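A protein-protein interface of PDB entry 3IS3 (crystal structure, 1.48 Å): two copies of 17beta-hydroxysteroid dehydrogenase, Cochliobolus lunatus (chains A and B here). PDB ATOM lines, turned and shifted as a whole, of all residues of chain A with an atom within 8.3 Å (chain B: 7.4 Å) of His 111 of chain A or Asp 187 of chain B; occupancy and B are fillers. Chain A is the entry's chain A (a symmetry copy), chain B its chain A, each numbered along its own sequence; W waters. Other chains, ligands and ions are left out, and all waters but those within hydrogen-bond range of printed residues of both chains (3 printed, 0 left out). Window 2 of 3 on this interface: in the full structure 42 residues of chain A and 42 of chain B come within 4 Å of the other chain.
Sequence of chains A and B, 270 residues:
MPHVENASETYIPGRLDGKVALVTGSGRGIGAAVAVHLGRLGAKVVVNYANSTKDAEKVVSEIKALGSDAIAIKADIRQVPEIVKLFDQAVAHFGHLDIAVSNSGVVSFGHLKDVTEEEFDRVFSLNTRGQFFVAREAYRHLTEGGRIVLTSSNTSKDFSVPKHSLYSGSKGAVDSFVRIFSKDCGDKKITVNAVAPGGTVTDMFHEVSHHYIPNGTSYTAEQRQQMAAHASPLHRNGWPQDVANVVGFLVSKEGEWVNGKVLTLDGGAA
Hydrophobic or aromatic side chains of chain B that line the printed part of chain A: Phe 132, Tyr 139 and Phe 181.
Hydrophobic or aromatic side chains of chain A within 4 Å of the printed part of chain B: His 111, Leu 112 and Val 115.
Along chain A the printed residues that touch a printed residue of chain B span positions 111 to 165.
Among the printed residues, no Asp or Glu carboxylate lies within 4 Å of a Lys or Arg side-chain nitrogen of the other chain.
No position is printed for both chains.
Of the 15 pairs that touch across the chains among the printed residues, none has its exchanged pair printed and touching as well.
Of the printed residues of chain A, Asp 187 of chain B touches His 111.
No residue of chain A comes within 4 Å of Gly 186 of chain B.
Printed residues of chain A within 4 Å of Arg 136 of chain B: Leu 112 and Val 115.
Printed residues of chain B within 4 Å of Lys 113 of chain A: Tyr 139.
Of the printed residues of chain B, Ser 165 of chain A touches Phe 132 and Phe 181.
Of the printed residues of chain A, Phe 132 of chain B touches Leu 112 (3.7 Å), Val 115 (3.7 Å) and Ser 165 (3.8 Å).
Of the printed residues of chain A, Asp 184 of chain B touches His 111, Leu 112, Pro 162 and Lys 163.
Asp 114 of chain A touches none of the printed residues of chain B.
The nearest residue of chain B that does not touch His 111 of chain A is Cys 185 of chain B (4.7 Å).
The nearest residue of chain A that does not touch Asp 187 of chain B is Lys 113 of chain A (5.4 Å).
The guanidinium group (NH1) of Arg 136 of chain B sits at hydrogen-bond distance from the backbone carbonyl oxygen (O) of Val 115 of chain A.
The side-chain carboxylate (OD2) of Asp 184 of chain B lies within hydrogen-bond range of the backbone NH (N) of Leu 112 of chain A (2.9 Å).
The side-chain carboxylate (OD2) of Asp 187 of chain B sits at hydrogen-bond distance from a ring nitrogen (NE2) of His 111 of chain A (2.9 Å).
The backbone carbonyl oxygen (O) of Asp 184 of chain B sits at hydrogen-bond distance from a ring nitrogen (NE2) of His 111 of chain A.
The side-chain carboxylate (OD1) of Asp 184 of chain B sits at hydrogen-bond distance from the backbone NH (N) of Lys 163 of chain A (2.9 Å).
Water W1 lies within hydrogen-bond range of OD2 of Asp 184 of chain B (2.6 Å), OG of Ser 165 of chain A (2.7 Å), O of Gly 110 of chain A (2.8 Å), N of His 164 of chain A (3.4 Å) and N of Leu 112 of chain A (3.5 Å).
Water W2 lies within hydrogen-bond range of the side-chain carboxylate (OD2) of Asp 187 of chain B (2.8 Å) and the side-chain amino group (NZ) of Lys 113 of chain A (2.8 Å).
Water W3 lies within hydrogen-bond range of the side-chain carboxylate of Asp 184 of chain B (2.9 Å) and the side-chain amino group of Lys 163 of chain A (3.0 Å).
Among the printed residues, pairs that only touch across the chains: His 111 of chain A with Tyr 139 of chain B (3.6 Å), Leu 112 of chain A with Phe 132 of chain B (3.7 Å), Leu 112 of chain A with Arg 136 of chain B (3.3 Å), Leu 112 of chain A with Phe 181 of chain B (3.7 Å), Leu 112 of chain A with Cys 185 of chain B (3.9 Å), Lys 113 of chain A with Tyr 139 of chain B (3.5 Å), Val 115 of chain A with Phe 132 of chain B (3.7 Å), Pro 162 of chain A with Asp 184 of chain B (3.8 Å), Ser 165 of chain A with Phe 132 of chain B (3.8 Å) and Ser 165 of chain A with Phe 181 of chain B (3.1 Å).
The backbone carbonyl oxygen (O) of Tyr 139 of chain B is in hydrogen-bond range of the side-chain amino group (NZ) of Lys 188 of chain B, at 2.8 Å.
A ring nitrogen (ND1) of His 111 of chain A lies within hydrogen-bond range of the backbone NH (N) of Lys 113 of chain A.
The backbone NH (N) of Ile 190 of chain B is in hydrogen-bond range of the backbone carbonyl oxygen (O) of Cys 185 of chain B (3.2 Å).
The backbone carbonyl oxygen of Lys 163 of chain A sits at hydrogen-bond distance from the backbone NH of Gly 110 of chain A (2.8 Å).
The side-chain carboxylate (OD1) of Asp 187 of chain B lies within hydrogen-bond range of the side-chain hydroxyl (OH) of Tyr 139 of chain B (2.4 Å).
The side-chain sulfur (SG) of Cys 185 of chain B lies close to the backbone carbonyl oxygen (O) of Phe 181 of chain B, 3.3 Å away.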
ATOM      1  N   SER A 108      14.287   3.226 -11.583  1.00  0.00           N
ATOM      2  CA  SER A 108      14.795   3.328 -10.219  1.00  0.00           C
ATOM      3  C   SER A 108      13.687   3.858  -9.335  1.00  0.00           C
ATOM      4  O   SER A 108      12.912   4.719  -9.764  1.00  0.00           O
ATOM      5  CB  SER A 108      15.969   4.320 -10.197  1.00  0.00           C
ATOM      6  OG  SER A 108      16.508   4.425  -8.889  1.00  0.00           O
ATOM      7  N   PHE A 109      13.641   3.356  -8.113  1.00  0.00           N
ATOM      8  CA  PHE A 109      12.686   3.810  -7.110  1.00  0.00           C
ATOM      9  C   PHE A 109      13.349   3.994  -5.778  1.00  0.00           C
ATOM     10  O   PHE A 109      14.188   3.160  -5.368  1.00  0.00           O
ATOM     11  CB  PHE A 109      11.507   2.827  -6.970  1.00  0.00           C
ATOM     12  CG  PHE A 109      10.850   2.511  -8.281  1.00  0.00           C
ATOM     13  CD1 PHE A 109      11.327   1.452  -9.071  1.00  0.00           C
ATOM     14  CD2 PHE A 109       9.797   3.277  -8.739  1.00  0.00           C
ATOM     15  CE1 PHE A 109      10.748   1.177 -10.307  1.00  0.00           C
ATOM     16  CE2 PHE A 109       9.202   3.004  -9.975  1.00  0.00           C
ATOM     17  CZ  PHE A 109       9.678   1.942 -10.751  1.00  0.00           C
ATOM     18  N   GLY A 110      12.874   4.992  -5.044  1.00  0.00           N
ATOM     19  CA  GLY A 110      13.284   5.179  -3.663  1.00  0.00           C
ATOM     20  C   GLY A 110      12.990   6.603  -3.226  1.00  0.00           C
ATOM     21  O   GLY A 110      13.052   7.524  -4.052  1.00  0.00           O
ATOM     22  N   HIS A 111      12.663   6.749  -1.946  1.00  0.00           N
ATOM     23  CA  HIS A 111      12.509   8.076  -1.363  1.00  0.00           C
ATOM     24  C   HIS A 111      13.826   8.847  -1.506  1.00  0.00           C
ATOM     25  O   HIS A 111      14.918   8.281  -1.357  1.00  0.00           O
ATOM     26  CB  HIS A 111      12.205   7.877   0.095  1.00  0.00           C
ATOM     27  CG  HIS A 111      11.721   9.090   0.831  1.00  0.00           C
ATOM     28  ND1 HIS A 111      12.515  10.189   1.079  1.00  0.00           N
ATOM     29  CD2 HIS A 111      10.528   9.350   1.413  1.00  0.00           C
ATOM     30  CE1 HIS A 111      11.837  11.064   1.805  1.00  0.00           C
ATOM     31  NE2 HIS A 111      10.623  10.580   2.021  1.00  0.00           N
ATOM     32  N   LEU A 112      13.696  10.145  -1.756  1.00  0.00           N
ATOM     33  CA  LEU A 112      14.854  11.067  -1.840  1.00  0.00           C
ATOM     34  C   LEU A 112      15.886  10.809  -0.739  1.00  0.00           C
ATOM     35  O   LEU A 112      17.087  10.765  -1.010  1.00  0.00           O
ATOM     36  CB  LEU A 112      14.367  12.508  -1.724  1.00  0.00           C
ATOM     37  CG  LEU A 112      15.446  13.584  -1.526  1.00  0.00           C
ATOM     38  CD1 LEU A 112      16.396  13.546  -2.712  1.00  0.00           C
ATOM     39  CD2 LEU A 112      14.732  14.969  -1.365  1.00  0.00           C
ATOM     40  N   LYS A 113      15.398  10.624   0.476  1.00  0.00           N
ATOM     41  CA  LYS A 113      16.255  10.491   1.687  1.00  0.00           C
ATOM     42  C   LYS A 113      17.285   9.369   1.551  1.00  0.00           C
ATOM     43  O   LYS A 113      18.330   9.437   2.203  1.00  0.00           O
ATOM     44  CB  LYS A 113      15.419  10.304   2.965  1.00  0.00           C
ATOM     45  CG  LYS A 113      14.807   8.909   3.125  1.00  0.00           C
ATOM     46  CD  LYS A 113      13.810   8.868   4.313  1.00  0.00           C
ATOM     47  CE  LYS A 113      13.230   7.452   4.537  1.00  0.00           C
ATOM     48  NZ  LYS A 113      12.346   7.384   5.756  1.00  0.00           N
ATOM     49  N   ASP A 114      16.957   8.361   0.745  1.00  0.00           N
ATOM     50  CA  ASP A 114      17.759   7.137   0.648  1.00  0.00           C
ATOM     51  C   ASP A 114      18.539   7.010  -0.647  1.00  0.00           C
ATOM     52  O   ASP A 114      19.249   6.005  -0.835  1.00  0.00           O
ATOM     53  CB  ASP A 114      16.876   5.878   0.763  1.00  0.00           C
ATOM     54  CG  ASP A 114      16.166   5.762   2.093  1.00  0.00           C
ATOM     55  OD1 ASP A 114      16.819   5.946   3.130  1.00  0.00           O
ATOM     56  OD2 ASP A 114      14.931   5.497   2.063  1.00  0.00           O
ATOM     57  N   VAL A 115      18.416   7.977  -1.555  1.00  0.00           N
ATOM     58  CA  VAL A 115      19.101   7.882  -2.839  1.00  0.00           C
ATOM     59  C   VAL A 115      20.592   8.097  -2.659  1.00  0.00           C
ATOM     60  O   VAL A 115      20.994   9.065  -2.033  1.00  0.00           O
ATOM     61  CB  VAL A 115      18.520   8.841  -3.885  1.00  0.00           C
ATOM     62  CG1 VAL A 115      19.296   8.727  -5.225  1.00  0.00           C
ATOM     63  CG2 VAL A 115      17.011   8.527  -4.089  1.00  0.00           C
ATOM     64  N   THR A 116      21.387   7.147  -3.152  1.00  0.00           N
ATOM     65  CA  THR A 116      22.846   7.204  -3.001  1.00  0.00           C
ATOM     66  C   THR A 116      23.487   7.869  -4.222  1.00  0.00           C
ATOM     67  O   THR A 116      22.902   7.944  -5.309  1.00  0.00           O
ATOM     68  CB  THR A 116      23.462   5.789  -2.867  1.00  0.00           C
ATOM     69  OG1 THR A 116      23.195   5.066  -4.074  1.00  0.00           O
ATOM     70  CG2 THR A 116      22.891   5.051  -1.650  1.00  0.00           C
ATOM     71  N   PRO A 162       5.302   9.080  -6.192  1.00  0.00           N
ATOM     72  CA  PRO A 162       6.185   9.252  -5.019  1.00  0.00           C
ATOM     73  C   PRO A 162       7.362   8.284  -5.142  1.00  0.00           C
ATOM     74  O   PRO A 162       7.239   7.186  -5.733  1.00  0.00           O
ATOM     75  CB  PRO A 162       5.293   8.898  -3.840  1.00  0.00           C
ATOM     76  CG  PRO A 162       3.873   9.156  -4.364  1.00  0.00           C
ATOM     77  CD  PRO A 162       3.916   8.767  -5.820  1.00  0.00           C
ATOM     78  N   LYS A 163       8.498   8.666  -4.566  1.00  0.00           N
ATOM     79  CA  LYS A 163       9.667   7.761  -4.559  1.00  0.00           C
ATOM     80  C   LYS A 163      10.189   7.464  -5.963  1.00  0.00           C
ATOM     81  O   LYS A 163      10.814   6.452  -6.206  1.00  0.00           O
ATOM     82  CB  LYS A 163       9.366   6.463  -3.742  1.00  0.00           C
ATOM     83  CG  LYS A 163       8.909   6.741  -2.321  1.00  0.00           C
ATOM     84  CD  LYS A 163       8.866   5.464  -1.484  1.00  0.00           C
ATOM     85  CE  LYS A 163       8.479   5.788  -0.049  1.00  0.00           C
ATOM     86  NZ  LYS A 163       7.078   6.292   0.076  1.00  0.00           N
ATOM     87  N   HIS A 164      10.003   8.409  -6.883  1.00  0.00           N
ATOM     88  CA  HIS A 164      10.456   8.210  -8.242  1.00  0.00           C
ATOM     89  C   HIS A 164      11.111   9.504  -8.757  1.00  0.00           C
ATOM     90  O   HIS A 164      11.135   9.756  -9.949  1.00  0.00           O
ATOM     91  CB  HIS A 164       9.208   7.808  -9.074  1.00  0.00           C
ATOM     92  CG  HIS A 164       9.493   7.142 -10.378  1.00  0.00           C
ATOM     93  ND1 HIS A 164      10.410   6.117 -10.531  1.00  0.00           N
ATOM     94  CD2 HIS A 164       8.866   7.262 -11.578  1.00  0.00           C
ATOM     95  CE1 HIS A 164      10.348   5.659 -11.771  1.00  0.00           C
ATOM     96  NE2 HIS A 164       9.405   6.320 -12.418  1.00  0.00           N
ATOM     97  N   SER A 165      11.730  10.253  -7.838  1.00  0.00           N
ATOM     98  CA  SER A 165      12.293  11.538  -8.237  1.00  0.00           C
ATOM     99  C   SER A 165      13.487  11.410  -9.160  1.00  0.00           C
ATOM    100  O   SER A 165      13.599  12.155 -10.127  1.00  0.00           O
ATOM    101  CB  SER A 165      12.663  12.388  -7.023  1.00  0.00           C
ATOM    102  OG  SER A 165      13.731  11.818  -6.285  1.00  0.00           O
ATOM    103  N   LEU A 166      14.378  10.459  -8.865  1.00  0.00           N
ATOM    104  CA  LEU A 166      15.602  10.315  -9.650  1.00  0.00           C
ATOM    105  C   LEU A 166      15.278   9.995 -11.109  1.00  0.00           C
ATOM    106  O   LEU A 166      15.783  10.648 -12.020  1.00  0.00           O
ATOM    107  CB  LEU A 166      16.486   9.238  -9.009  1.00  0.00           C
ATOM    108  CG  LEU A 166      17.782   8.944  -9.722  1.00  0.00           C
ATOM    109  CD1 LEU A 166      18.706  10.202  -9.649  1.00  0.00           C
ATOM    110  CD2 LEU A 166      18.439   7.766  -9.027  1.00  0.00           C
ATOM    111  N   PHE B 132      20.420  17.980  -6.542  1.00  0.00           N
ATOM    112  CA  PHE B 132      19.667  16.801  -6.064  1.00  0.00           C
ATOM    113  C   PHE B 132      20.140  16.484  -4.650  1.00  0.00           C
ATOM    114  O   PHE B 132      19.324  16.264  -3.747  1.00  0.00           O
ATOM    115  CB  PHE B 132      19.955  15.607  -6.971  1.00  0.00           C
ATOM    116  CG  PHE B 132      19.215  14.364  -6.579  1.00  0.00           C
ATOM    117  CD1 PHE B 132      19.688  13.529  -5.563  1.00  0.00           C
ATOM    118  CD2 PHE B 132      18.001  14.051  -7.204  1.00  0.00           C
ATOM    119  CE1 PHE B 132      19.007  12.376  -5.187  1.00  0.00           C
ATOM    120  CE2 PHE B 132      17.310  12.895  -6.834  1.00  0.00           C
ATOM    121  CZ  PHE B 132      17.805  12.060  -5.813  1.00  0.00           C
ATOM    122  N   ARG B 136      18.561  16.354  -0.914  1.00  0.00           N
ATOM    123  CA  ARG B 136      18.593  15.185  -0.034  1.00  0.00           C
ATOM    124  C   ARG B 136      19.056  15.543   1.378  1.00  0.00           C
ATOM    125  O   ARG B 136      18.437  15.131   2.388  1.00  0.00           O
ATOM    126  CB  ARG B 136      19.526  14.115  -0.590  1.00  0.00           C
ATOM    127  CG  ARG B 136      19.381  12.798   0.177  1.00  0.00           C
ATOM    128  CD  ARG B 136      20.489  11.839  -0.171  1.00  0.00           C
ATOM    129  NE  ARG B 136      21.767  12.225   0.481  1.00  0.00           N
ATOM    130  CZ  ARG B 136      22.889  11.516   0.375  1.00  0.00           C
ATOM    131  NH1 ARG B 136      22.937  10.410  -0.366  1.00  0.00           N
ATOM    132  NH2 ARG B 136      23.991  11.934   0.999  1.00  0.00           N
ATOM    133  N   TYR B 139      16.408  17.622   3.191  1.00  0.00           N
ATOM    134  CA  TYR B 139      15.354  16.778   3.737  1.00  0.00           C
ATOM    135  C   TYR B 139      15.804  16.128   5.043  1.00  0.00           C
ATOM    136  O   TYR B 139      15.077  16.130   6.046  1.00  0.00           O
ATOM    137  CB  TYR B 139      14.903  15.683   2.750  1.00  0.00           C
ATOM    138  CG  TYR B 139      13.957  14.724   3.422  1.00  0.00           C
ATOM    139  CD1 TYR B 139      12.581  15.000   3.513  1.00  0.00           C
ATOM    140  CD2 TYR B 139      14.446  13.575   4.052  1.00  0.00           C
ATOM    141  CE1 TYR B 139      11.724  14.120   4.195  1.00  0.00           C
ATOM    142  CE2 TYR B 139      13.591  12.700   4.753  1.00  0.00           C
ATOM    143  CZ  TYR B 139      12.240  12.967   4.780  1.00  0.00           C
ATOM    144  OH  TYR B 139      11.428  12.090   5.470  1.00  0.00           O
ATOM    145  N   GLU B 144      10.655  19.983  10.812  1.00  0.00           N
ATOM    146  CA  GLU B 144       9.301  19.827  10.257  1.00  0.00           C
ATOM    147  C   GLU B 144       8.713  21.163   9.863  1.00  0.00           C
ATOM    148  O   GLU B 144       8.832  22.140  10.592  1.00  0.00           O
ATOM    149  CB  GLU B 144       8.393  19.231  11.335  1.00  0.00           C
ATOM    150  CG  GLU B 144       8.752  17.846  11.762  1.00  0.00           C
ATOM    151  CD  GLU B 144       8.040  16.792  10.930  1.00  0.00           C
ATOM    152  OE1 GLU B 144       6.868  17.021  10.531  1.00  0.00           O
ATOM    153  OE2 GLU B 144       8.649  15.729  10.699  1.00  0.00           O
ATOM    154  N   PHE B 181      10.036  15.556  -5.414  1.00  0.00           N
ATOM    155  CA  PHE B 181      10.545  15.820  -4.052  1.00  0.00           C
ATOM    156  C   PHE B 181       9.445  16.305  -3.159  1.00  0.00           C
ATOM    157  O   PHE B 181       9.422  15.994  -1.967  1.00  0.00           O
ATOM    158  CB  PHE B 181      11.607  16.927  -4.084  1.00  0.00           C
ATOM    159  CG  PHE B 181      12.949  16.526  -4.675  1.00  0.00           C
ATOM    160  CD1 PHE B 181      13.147  15.177  -4.981  1.00  0.00           C
ATOM    161  CD2 PHE B 181      13.969  17.447  -4.942  1.00  0.00           C
ATOM    162  CE1 PHE B 181      14.330  14.731  -5.540  1.00  0.00           C
ATOM    163  CE2 PHE B 181      15.194  17.007  -5.519  1.00  0.00           C
ATOM    164  CZ  PHE B 181      15.353  15.650  -5.832  1.00  0.00           C
ATOM    165  N   SER B 182       8.505  17.077  -3.701  1.00  0.00           N
ATOM    166  CA  SER B 182       7.418  17.563  -2.855  1.00  0.00           C
ATOM    167  C   SER B 182       6.582  16.420  -2.282  1.00  0.00           C
ATOM    168  O   SER B 182       6.068  16.517  -1.171  1.00  0.00           O
ATOM    169  CB  SER B 182       6.535  18.590  -3.605  1.00  0.00           C
ATOM    170  OG  SER B 182       5.677  17.983  -4.567  1.00  0.00           O
ATOM    171  N   LYS B 183       6.474  15.332  -3.039  1.00  0.00           N
ATOM    172  CA  LYS B 183       5.764  14.171  -2.535  1.00  0.00           C
ATOM    173  C   LYS B 183       6.535  13.541  -1.358  1.00  0.00           C
ATOM    174  O   LYS B 183       5.982  13.371  -0.248  1.00  0.00           O
ATOM    175  CB  LYS B 183       5.494  13.148  -3.645  1.00  0.00           C
ATOM    176  CG  LYS B 183       4.889  13.728  -4.959  1.00  0.00           C
ATOM    177  CD  LYS B 183       3.575  14.449  -4.666  1.00  0.00           C
ATOM    178  CE  LYS B 183       2.930  15.024  -5.971  1.00  0.00           C
ATOM    179  NZ  LYS B 183       3.638  16.347  -6.334  1.00  0.00           N
ATOM    180  N   ASP B 184       7.813  13.241  -1.590  1.00  0.00           N
ATOM    181  CA  ASP B 184       8.606  12.569  -0.540  1.00  0.00           C
ATOM    182  C   ASP B 184       8.786  13.456   0.701  1.00  0.00           C
ATOM    183  O   ASP B 184       8.710  12.987   1.854  1.00  0.00           O
ATOM    184  CB  ASP B 184       9.985  12.216  -1.087  1.00  0.00           C
ATOM    185  CG  ASP B 184       9.949  11.190  -2.187  1.00  0.00           C
ATOM    186  OD1 ASP B 184       8.870  10.651  -2.516  1.00  0.00           O
ATOM    187  OD2 ASP B 184      11.042  10.922  -2.727  1.00  0.00           O
ATOM    188  N   CYS B 185       9.020  14.745   0.471  1.00  0.00           N
ATOM    189  CA  CYS B 185       9.344  15.664   1.563  1.00  0.00           C
ATOM    190  C   CYS B 185       8.130  16.047   2.379  1.00  0.00           C
ATOM    191  O   CYS B 185       8.270  16.540   3.504  1.00  0.00           O
ATOM    192  CB  CYS B 185      10.037  16.928   1.002  1.00  0.00           C
ATOM    193  SG  CYS B 185      11.691  16.576   0.384  1.00  0.00           S
ATOM    194  N   GLY B 186       6.935  15.779   1.848  1.00  0.00           N
ATOM    195  CA  GLY B 186       5.710  16.035   2.609  1.00  0.00           C
ATOM    196  C   GLY B 186       5.630  15.262   3.919  1.00  0.00           C
ATOM    197  O   GLY B 186       4.905  15.642   4.842  1.00  0.00           O
ATOM    198  N   ASP B 187       6.394  14.180   4.015  1.00  0.00           N
ATOM    199  CA  ASP B 187       6.390  13.448   5.275  1.00  0.00           C
ATOM    200  C   ASP B 187       7.028  14.175   6.485  1.00  0.00           C
ATOM    201  O   ASP B 187       6.842  13.769   7.640  1.00  0.00           O
ATOM    202  CB  ASP B 187       6.762  11.962   5.093  1.00  0.00           C
ATOM    203  CG  ASP B 187       8.197  11.730   4.792  1.00  0.00           C
ATOM    204  OD1 ASP B 187       9.031  12.495   5.304  1.00  0.00           O
ATOM    205  OD2 ASP B 187       8.496  10.743   4.039  1.00  0.00           O
ATOM    206  N   LYS B 188       7.725  15.268   6.201  1.00  0.00           N
ATOM    207  CA  LYS B 188       8.212  16.185   7.229  1.00  0.00           C
ATOM    208  C   LYS B 188       7.563  17.562   7.043  1.00  0.00           C
ATOM    209  O   LYS B 188       8.031  18.560   7.584  1.00  0.00           O
ATOM    210  CB  LYS B 188       9.741  16.274   7.146  1.00  0.00           C
ATOM    211  CG  LYS B 188      10.437  14.990   7.653  1.00  0.00           C
ATOM    212  CD  LYS B 188      11.981  15.060   7.620  1.00  0.00           C
ATOM    213  CE  LYS B 188      12.538  16.156   8.478  1.00  0.00           C
ATOM    214  NZ  LYS B 188      14.060  16.078   8.601  1.00  0.00           N
ATOM    215  N   LYS B 189       6.487  17.603   6.239  1.00  0.00           N
ATOM    216  CA  LYS B 189       5.754  18.859   5.945  1.00  0.00           C
ATOM    217  C   LYS B 189       6.686  19.937   5.351  1.00  0.00           C
ATOM    218  O   LYS B 189       6.493  21.138   5.559  1.00  0.00           O
ATOM    219  CB  LYS B 189       4.957  19.350   7.169  1.00  0.00           C
ATOM    220  CG  LYS B 189       4.076  18.280   7.820  1.00  0.00           C
ATOM    221  CD  LYS B 189       2.899  17.915   6.970  1.00  0.00           C
ATOM    222  CE  LYS B 189       1.838  17.140   7.794  1.00  0.00           C
ATOM    223  NZ  LYS B 189       2.242  15.724   8.065  1.00  0.00           N
ATOM    224  N   ILE B 190       7.678  19.486   4.580  1.00  0.00           N
ATOM    225  CA  ILE B 190       8.625  20.379   3.909  1.00  0.00           C
ATOM    226  C   ILE B 190       8.109  20.607   2.497  1.00  0.00           C
ATOM    227  O   ILE B 190       7.827  19.655   1.781  1.00  0.00           O
ATOM    228  CB  ILE B 190      10.022  19.728   3.845  1.00  0.00           C
ATOM    229  CG1 ILE B 190      10.577  19.625   5.295  1.00  0.00           C
ATOM    230  CG2 ILE B 190      10.960  20.549   2.940  1.00  0.00           C
ATOM    231  CD1 ILE B 190      11.805  18.728   5.373  1.00  0.00           C
HETATM  232  O   HOH W   1      12.201  10.045  -4.915  1.00  0.00           O
HETATM  233  O   HOH W   2       9.900   8.646   5.148  1.00  0.00           O
HETATM  234  O   HOH W   3       7.212   9.234  -0.624  1.00  0.00           O
